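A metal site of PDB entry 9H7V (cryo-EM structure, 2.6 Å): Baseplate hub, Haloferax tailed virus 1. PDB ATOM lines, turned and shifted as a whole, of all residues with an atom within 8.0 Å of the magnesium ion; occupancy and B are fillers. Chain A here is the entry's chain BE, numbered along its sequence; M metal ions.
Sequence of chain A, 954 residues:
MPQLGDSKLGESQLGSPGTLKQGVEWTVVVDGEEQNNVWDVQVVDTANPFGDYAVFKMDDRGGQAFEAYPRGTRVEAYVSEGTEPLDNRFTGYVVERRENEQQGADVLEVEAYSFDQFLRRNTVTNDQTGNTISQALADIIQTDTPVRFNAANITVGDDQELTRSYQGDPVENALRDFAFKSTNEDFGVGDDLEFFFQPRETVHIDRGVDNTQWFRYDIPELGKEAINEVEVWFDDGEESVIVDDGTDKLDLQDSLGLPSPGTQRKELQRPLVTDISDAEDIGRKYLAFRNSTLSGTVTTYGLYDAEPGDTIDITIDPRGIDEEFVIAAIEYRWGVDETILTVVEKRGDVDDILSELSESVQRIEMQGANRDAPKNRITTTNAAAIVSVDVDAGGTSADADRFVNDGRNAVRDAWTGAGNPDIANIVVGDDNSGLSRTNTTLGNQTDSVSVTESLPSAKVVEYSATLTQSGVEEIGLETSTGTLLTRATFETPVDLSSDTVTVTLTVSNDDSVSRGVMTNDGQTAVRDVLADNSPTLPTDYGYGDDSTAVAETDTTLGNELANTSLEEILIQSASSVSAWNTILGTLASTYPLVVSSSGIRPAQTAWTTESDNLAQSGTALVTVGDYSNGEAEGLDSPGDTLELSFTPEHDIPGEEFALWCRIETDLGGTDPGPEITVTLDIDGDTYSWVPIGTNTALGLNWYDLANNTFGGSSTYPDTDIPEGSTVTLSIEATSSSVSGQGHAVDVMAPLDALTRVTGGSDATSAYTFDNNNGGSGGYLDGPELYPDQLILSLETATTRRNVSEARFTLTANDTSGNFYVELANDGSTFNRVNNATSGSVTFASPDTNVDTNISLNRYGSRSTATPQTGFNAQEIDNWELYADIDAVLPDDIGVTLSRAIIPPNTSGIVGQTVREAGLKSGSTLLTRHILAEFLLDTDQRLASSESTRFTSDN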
ATOM      1  N   THR A 609      25.497  10.145  -6.011  1.00  0.00           N
ATOM      2  CA  THR A 609      26.170  10.007  -7.294  1.00  0.00           C
ATOM      3  C   THR A 609      25.593   8.823  -8.056  1.00  0.00           C
ATOM      4  O   THR A 609      25.416   7.746  -7.489  1.00  0.00           O
ATOM      5  CB  THR A 609      27.690   9.860  -7.089  1.00  0.00           C
ATOM      6  OG1 THR A 609      28.130  10.919  -6.238  1.00  0.00           O
ATOM      7  CG2 THR A 609      28.477   9.880  -8.376  1.00  0.00           C
ATOM      8  N   GLU A 610      25.323   9.044  -9.351  1.00  0.00           N
ATOM      9  CA  GLU A 610      24.807   8.011 -10.229  1.00  0.00           C
ATOM     10  C   GLU A 610      25.927   7.073 -10.669  1.00  0.00           C
ATOM     11  O   GLU A 610      27.096   7.467 -10.736  1.00  0.00           O
ATOM     12  CB  GLU A 610      24.156   8.643 -11.460  1.00  0.00           C
ATOM     13  CG  GLU A 610      22.666   8.822 -11.286  1.00  0.00           C
ATOM     14  CD  GLU A 610      21.769   7.716 -11.822  1.00  0.00           C
ATOM     15  OE1 GLU A 610      22.125   6.504 -11.709  1.00  0.00           O
ATOM     16  OE2 GLU A 610      20.706   8.073 -12.358  1.00  0.00           O
ATOM     17  N   SER A 611      25.509   5.832 -10.960  1.00  0.00           N
ATOM     18  CA  SER A 611      26.234   4.808 -11.710  1.00  0.00           C
ATOM     19  C   SER A 611      27.146   5.420 -12.783  1.00  0.00           C
ATOM     20  O   SER A 611      28.309   5.043 -12.887  1.00  0.00           O
ATOM     21  CB  SER A 611      25.240   3.844 -12.323  1.00  0.00           C
ATOM     22  OG  SER A 611      24.044   4.514 -12.728  1.00  0.00           O
ATOM     23  N   ASP A 612      26.581   6.358 -13.547  1.00  0.00           N
ATOM     24  CA  ASP A 612      27.169   7.005 -14.715  1.00  0.00           C
ATOM     25  C   ASP A 612      28.458   7.745 -14.340  1.00  0.00           C
ATOM     26  O   ASP A 612      29.444   7.661 -15.071  1.00  0.00           O
ATOM     27  CB  ASP A 612      26.118   7.917 -15.353  1.00  0.00           C
ATOM     28  CG  ASP A 612      26.527   8.648 -16.630  1.00  0.00           C
ATOM     29  OD1 ASP A 612      27.489   8.206 -17.302  1.00  0.00           O
ATOM     30  OD2 ASP A 612      25.858   9.649 -16.955  1.00  0.00           O
ATOM     31  N   ASN A 613      28.451   8.429 -13.185  1.00  0.00           N
ATOM     32  CA  ASN A 613      29.443   9.445 -12.864  1.00  0.00           C
ATOM     33  C   ASN A 613      30.599   8.893 -12.031  1.00  0.00           C
ATOM     34  O   ASN A 613      31.634   9.547 -11.943  1.00  0.00           O
ATOM     35  CB  ASN A 613      28.810  10.676 -12.202  1.00  0.00           C
ATOM     36  CG  ASN A 613      27.894  11.455 -13.115  1.00  0.00           C
ATOM     37  OD1 ASN A 613      26.682  11.466 -12.922  1.00  0.00           O
ATOM     38  ND2 ASN A 613      28.462  12.113 -14.111  1.00  0.00           N
ATOM     39  N   LEU A 614      30.412   7.707 -11.426  1.00  0.00           N
ATOM     40  CA  LEU A 614      31.441   7.091 -10.584  1.00  0.00           C
ATOM     41  C   LEU A 614      32.670   6.764 -11.414  1.00  0.00           C
ATOM     42  O   LEU A 614      32.550   6.429 -12.595  1.00  0.00           O
ATOM     43  CB  LEU A 614      30.867   5.811  -9.953  1.00  0.00           C
ATOM     44  CG  LEU A 614      29.758   5.994  -8.922  1.00  0.00           C
ATOM     45  CD1 LEU A 614      28.968   4.702  -8.735  1.00  0.00           C
ATOM     46  CD2 LEU A 614      30.305   6.486  -7.582  1.00  0.00           C
ATOM     47  N   VAL A 622      25.088  -2.578 -16.819  1.00  0.00           N
ATOM     48  CA  VAL A 622      23.813  -3.287 -16.762  1.00  0.00           C
ATOM     49  C   VAL A 622      22.712  -2.292 -17.126  1.00  0.00           C
ATOM     50  O   VAL A 622      22.633  -1.227 -16.511  1.00  0.00           O
ATOM     51  CB  VAL A 622      23.578  -3.940 -15.387  1.00  0.00           C
ATOM     52  CG1 VAL A 622      22.402  -4.919 -15.410  1.00  0.00           C
ATOM     53  CG2 VAL A 622      24.813  -4.633 -14.837  1.00  0.00           C
ATOM     54  N   VAL A 624      18.695  -1.645 -17.325  1.00  0.00           N
ATOM     55  CA  VAL A 624      17.386  -2.067 -16.811  1.00  0.00           C
ATOM     56  C   VAL A 624      16.502  -0.832 -16.633  1.00  0.00           C
ATOM     57  O   VAL A 624      16.983   0.220 -16.228  1.00  0.00           O
ATOM     58  CB  VAL A 624      17.500  -2.854 -15.496  1.00  0.00           C
ATOM     59  CG1 VAL A 624      16.200  -3.565 -15.128  1.00  0.00           C
ATOM     60  CG2 VAL A 624      18.642  -3.863 -15.489  1.00  0.00           C
ATOM     61  N   ASP A 626      14.343  -0.162 -14.377  1.00  0.00           N
ATOM     62  CA  ASP A 626      14.081   0.177 -12.991  1.00  0.00           C
ATOM     63  C   ASP A 626      15.254   0.909 -12.354  1.00  0.00           C
ATOM     64  O   ASP A 626      15.139   1.404 -11.225  1.00  0.00           O
ATOM     65  CB  ASP A 626      13.676  -1.062 -12.182  1.00  0.00           C
ATOM     66  CG  ASP A 626      12.348  -1.685 -12.594  1.00  0.00           C
ATOM     67  OD1 ASP A 626      11.501  -0.971 -13.178  1.00  0.00           O
ATOM     68  OD2 ASP A 626      12.172  -2.894 -12.332  1.00  0.00           O
ATOM     69  N   TYR A 627      16.391   0.975 -13.063  1.00  0.00           N
ATOM     70  CA  TYR A 627      17.578   1.631 -12.531  1.00  0.00           C
ATOM     71  C   TYR A 627      17.518   3.130 -12.832  1.00  0.00           C
ATOM     72  O   TYR A 627      16.922   3.554 -13.816  1.00  0.00           O
ATOM     73  CB  TYR A 627      18.865   1.005 -13.073  1.00  0.00           C
ATOM     74  CG  TYR A 627      19.123  -0.429 -12.709  1.00  0.00           C
ATOM     75  CD1 TYR A 627      18.412  -1.077 -11.694  1.00  0.00           C
ATOM     76  CD2 TYR A 627      20.107  -1.161 -13.358  1.00  0.00           C
ATOM     77  CE1 TYR A 627      18.655  -2.395 -11.362  1.00  0.00           C
ATOM     78  CE2 TYR A 627      20.379  -2.478 -13.027  1.00  0.00           C
ATOM     79  CZ  TYR A 627      19.640  -3.103 -12.029  1.00  0.00           C
ATOM     80  OH  TYR A 627      19.901  -4.401 -11.701  1.00  0.00           O
ATOM     81  N   SER A 628      18.156   3.910 -11.956  1.00  0.00           N
ATOM     82  CA  SER A 628      18.317   5.343 -12.123  1.00  0.00           C
ATOM     83  C   SER A 628      19.311   5.607 -13.260  1.00  0.00           C
ATOM     84  O   SER A 628      20.479   5.210 -13.180  1.00  0.00           O
ATOM     85  CB  SER A 628      18.756   5.985 -10.827  1.00  0.00           C
ATOM     86  OG  SER A 628      18.617   7.400 -10.888  1.00  0.00           O
ATOM     87  N   ASN A 629      18.773   6.278 -14.294  1.00  0.00           N
ATOM     88  CA  ASN A 629      19.340   6.526 -15.613  1.00  0.00           C
ATOM     89  C   ASN A 629      19.311   5.258 -16.469  1.00  0.00           C
ATOM     90  O   ASN A 629      20.001   5.179 -17.481  1.00  0.00           O
ATOM     91  CB  ASN A 629      20.708   7.224 -15.557  1.00  0.00           C
ATOM     92  CG  ASN A 629      20.959   8.167 -16.727  1.00  0.00           C
ATOM     93  OD1 ASN A 629      21.227   9.343 -16.511  1.00  0.00           O
ATOM     94  ND2 ASN A 629      20.899   7.668 -17.947  1.00  0.00           N
ATOM     95  N   GLY A 630      18.480   4.285 -16.062  1.00  0.00           N
ATOM     96  CA  GLY A 630      18.373   2.996 -16.736  1.00  0.00           C
ATOM     97  C   GLY A 630      19.685   2.216 -16.707  1.00  0.00           C
ATOM     98  O   GLY A 630      19.880   1.309 -17.523  1.00  0.00           O
ATOM     99  N   GLU A 631      20.550   2.568 -15.748  1.00  0.00           N
ATOM    100  CA  GLU A 631      21.973   2.242 -15.769  1.00  0.00           C
ATOM    101  C   GLU A 631      22.501   2.017 -14.343  1.00  0.00           C
ATOM    102  O   GLU A 631      22.267   2.834 -13.440  1.00  0.00           O
ATOM    103  CB  GLU A 631      22.723   3.337 -16.524  1.00  0.00           C
ATOM    104  CG  GLU A 631      24.231   3.335 -16.339  1.00  0.00           C
ATOM    105  CD  GLU A 631      25.013   4.261 -17.264  1.00  0.00           C
ATOM    106  OE1 GLU A 631      24.388   5.055 -18.001  1.00  0.00           O
ATOM    107  OE2 GLU A 631      26.260   4.178 -17.251  1.00  0.00           O
ATOM    108  N   ALA A 632      23.243   0.902 -14.204  1.00  0.00           N
ATOM    109  CA  ALA A 632      23.967   0.506 -13.015  1.00  0.00           C
ATOM    110  C   ALA A 632      25.257  -0.220 -13.385  1.00  0.00           C
ATOM    111  O   ALA A 632      25.362  -0.802 -14.469  1.00  0.00           O
ATOM    112  CB  ALA A 632      23.106  -0.357 -12.135  1.00  0.00           C
ATOM    113  N   GLU A 633      26.229  -0.212 -12.454  1.00  0.00           N
ATOM    114  CA  GLU A 633      27.554  -0.773 -12.654  1.00  0.00           C
ATOM    115  C   GLU A 633      27.687  -2.094 -11.894  1.00  0.00           C
ATOM    116  O   GLU A 633      27.585  -2.111 -10.670  1.00  0.00           O
ATOM    117  CB  GLU A 633      28.627   0.226 -12.205  1.00  0.00           C
ATOM    118  CG  GLU A 633      28.859   1.349 -13.190  1.00  0.00           C
ATOM    119  CD  GLU A 633      29.267   0.919 -14.590  1.00  0.00           C
ATOM    120  OE1 GLU A 633      30.127   0.026 -14.713  1.00  0.00           O
ATOM    121  OE2 GLU A 633      28.694   1.473 -15.556  1.00  0.00           O
ATOM    122  N   ARG A 662      21.805   1.912  -3.894  1.00  0.00           N
ATOM    123  CA  ARG A 662      20.871   1.043  -4.575  1.00  0.00           C
ATOM    124  C   ARG A 662      21.664  -0.112  -5.188  1.00  0.00           C
ATOM    125  O   ARG A 662      22.544   0.106  -6.022  1.00  0.00           O
ATOM    126  CB  ARG A 662      20.094   1.777  -5.666  1.00  0.00           C
ATOM    127  CG  ARG A 662      18.881   2.536  -5.143  1.00  0.00           C
ATOM    128  CD  ARG A 662      18.014   2.964  -6.308  1.00  0.00           C
ATOM    129  NE  ARG A 662      16.732   2.275  -6.356  1.00  0.00           N
ATOM    130  CZ  ARG A 662      16.078   1.956  -7.465  1.00  0.00           C
ATOM    131  NH1 ARG A 662      14.908   1.340  -7.387  1.00  0.00           N
ATOM    132  NH2 ARG A 662      16.581   2.236  -8.654  1.00  0.00           N
ATOM    133  N   VAL A 745      25.461  -1.591  -8.948  1.00  0.00           N
ATOM    134  CA  VAL A 745      25.386  -0.353  -8.173  1.00  0.00           C
ATOM    135  C   VAL A 745      24.753   0.721  -9.043  1.00  0.00           C
ATOM    136  O   VAL A 745      25.319   1.122 -10.052  1.00  0.00           O
ATOM    137  CB  VAL A 745      26.771   0.078  -7.639  1.00  0.00           C
ATOM    138  CG1 VAL A 745      26.724   1.408  -6.907  1.00  0.00           C
ATOM    139  CG2 VAL A 745      27.389  -0.995  -6.740  1.00  0.00           C
ATOM    140  N   ASP A 746      23.572   1.201  -8.619  1.00  0.00           N
ATOM    141  CA  ASP A 746      22.723   2.036  -9.447  1.00  0.00           C
ATOM    142  C   ASP A 746      22.906   3.520  -9.143  1.00  0.00           C
ATOM    143  O   ASP A 746      22.903   4.333 -10.081  1.00  0.00           O
ATOM    144  CB  ASP A 746      21.249   1.629  -9.355  1.00  0.00           C
ATOM    145  CG  ASP A 746      20.297   2.594 -10.043  1.00  0.00           C
ATOM    146  OD1 ASP A 746      20.711   3.204 -11.060  1.00  0.00           O
ATOM    147  OD2 ASP A 746      19.153   2.736  -9.570  1.00  0.00           O
ATOM    148  N   VAL A 747      22.945   3.815  -7.828  1.00  0.00           N
ATOM    149  CA  VAL A 747      23.180   5.113  -7.192  1.00  0.00           C
ATOM    150  C   VAL A 747      23.940   4.850  -5.880  1.00  0.00           C
ATOM    151  O   VAL A 747      23.587   3.953  -5.125  1.00  0.00           O
ATOM    152  CB  VAL A 747      21.874   5.877  -6.890  1.00  0.00           C
ATOM    153  CG1 VAL A 747      22.140   7.260  -6.309  1.00  0.00           C
ATOM    154  CG2 VAL A 747      20.949   5.997  -8.088  1.00  0.00           C
ATOM    155  N   MET A 748      24.971   5.675  -5.624  1.00  0.00           N
ATOM    156  CA  MET A 748      25.771   5.615  -4.417  1.00  0.00           C
ATOM    157  C   MET A 748      25.661   6.948  -3.669  1.00  0.00           C
ATOM    158  O   MET A 748      25.880   8.009  -4.258  1.00  0.00           O
ATOM    159  CB  MET A 748      27.232   5.337  -4.752  1.00  0.00           C
ATOM    160  CG  MET A 748      28.080   4.924  -3.559  1.00  0.00           C
ATOM    161  SD  MET A 748      29.837   4.755  -3.963  1.00  0.00           S
ATOM    162  CE  MET A 748      29.785   3.450  -5.194  1.00  0.00           C
ATOM    163  N   ASN A 773      11.221   4.230  -9.892  1.00  0.00           N
ATOM    164  CA  ASN A 773      11.896   4.867 -11.005  1.00  0.00           C
ATOM    165  C   ASN A 773      10.875   5.289 -12.059  1.00  0.00           C
ATOM    166  O   ASN A 773      11.129   6.204 -12.836  1.00  0.00           O
ATOM    167  CB  ASN A 773      12.959   3.956 -11.604  1.00  0.00           C
ATOM    168  CG  ASN A 773      13.852   4.660 -12.612  1.00  0.00           C
ATOM    169  OD1 ASN A 773      13.608   4.594 -13.813  1.00  0.00           O
ATOM    170  ND2 ASN A 773      14.879   5.349 -12.122  1.00  0.00           N
ATOM    171  N   GLY A 777      13.787   3.987 -17.033  1.00  0.00           N
ATOM    172  CA  GLY A 777      15.154   4.470 -16.977  1.00  0.00           C
ATOM    173  C   GLY A 777      15.241   5.944 -16.594  1.00  0.00           C
ATOM    174  O   GLY A 777      16.175   6.645 -16.999  1.00  0.00           O
ATOM    175  N   GLY A 778      14.262   6.401 -15.799  1.00  0.00           N
ATOM    176  CA  GLY A 778      14.194   7.757 -15.287  1.00  0.00           C
ATOM    177  C   GLY A 778      15.035   7.946 -14.025  1.00  0.00           C
ATOM    178  O   GLY A 778      16.097   7.339 -13.882  1.00  0.00           O
ATOM    179  N   TYR A 779      14.524   8.789 -13.115  1.00  0.00           N
ATOM    180  CA  TYR A 779      15.294   9.292 -11.976  1.00  0.00           C
ATOM    181  C   TYR A 779      14.471   9.226 -10.692  1.00  0.00           C
ATOM    182  O   TYR A 779      13.247   9.083 -10.741  1.00  0.00           O
ATOM    183  CB  TYR A 779      15.798  10.704 -12.279  1.00  0.00           C
ATOM    184  CG  TYR A 779      16.707  10.817 -13.478  1.00  0.00           C
ATOM    185  CD1 TYR A 779      18.044  10.438 -13.400  1.00  0.00           C
ATOM    186  CD2 TYR A 779      16.236  11.285 -14.691  1.00  0.00           C
ATOM    187  CE1 TYR A 779      18.886  10.539 -14.498  1.00  0.00           C
ATOM    188  CE2 TYR A 779      17.060  11.390 -15.803  1.00  0.00           C
ATOM    189  CZ  TYR A 779      18.389  11.014 -15.704  1.00  0.00           C
ATOM    190  OH  TYR A 779      19.215  11.103 -16.793  1.00  0.00           O
ATOM    191  N   LEU A 780      15.171   9.342  -9.554  1.00  0.00           N
ATOM    192  CA  LEU A 780      14.596   9.164  -8.220  1.00  0.00           C
ATOM    193  C   LEU A 780      14.627  10.485  -7.467  1.00  0.00           C
ATOM    194  O   LEU A 780      15.589  11.245  -7.592  1.00  0.00           O
ATOM    195  CB  LEU A 780      15.428   8.124  -7.455  1.00  0.00           C
ATOM    196  CG  LEU A 780      15.611   6.761  -8.126  1.00  0.00           C
ATOM    197  CD1 LEU A 780      16.847   6.068  -7.576  1.00  0.00           C
ATOM    198  CD2 LEU A 780      14.380   5.884  -7.938  1.00  0.00           C
ATOM    199  N   THR A 866      19.268  12.394 -10.644  1.00  0.00           N
ATOM    200  CA  THR A 866      19.065  11.935  -9.276  1.00  0.00           C
ATOM    201  C   THR A 866      20.108  12.635  -8.385  1.00  0.00           C
ATOM    202  O   THR A 866      21.290  12.589  -8.718  1.00  0.00           O
ATOM    203  CB  THR A 866      19.167  10.405  -9.188  1.00  0.00           C
ATOM    204  OG1 THR A 866      18.067   9.852  -9.897  1.00  0.00           O
ATOM    205  CG2 THR A 866      19.168   9.865  -7.772  1.00  0.00           C
HETATM  206 MG    MG M   1      21.903   4.556 -12.052  1.00  0.00          MG
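OG1 of Thr 866 sits at hydrogen-bond distance from OG of Ser 628.
OE2 of Glu 610 is in hydrogen-bond range of N of Asn 629, 3.3 Å away.
The side-chain carboxylate (OD2) of Asp 746 lies within salt-bridge range of the guanidinium group (NH2) of Arg 662.
The magnesium ion is bound by O of Ser 628, OE1 of Glu 610, OD1 of Asp 746, O of Asp 746, O of Glu 631 and OG of Ser 611.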
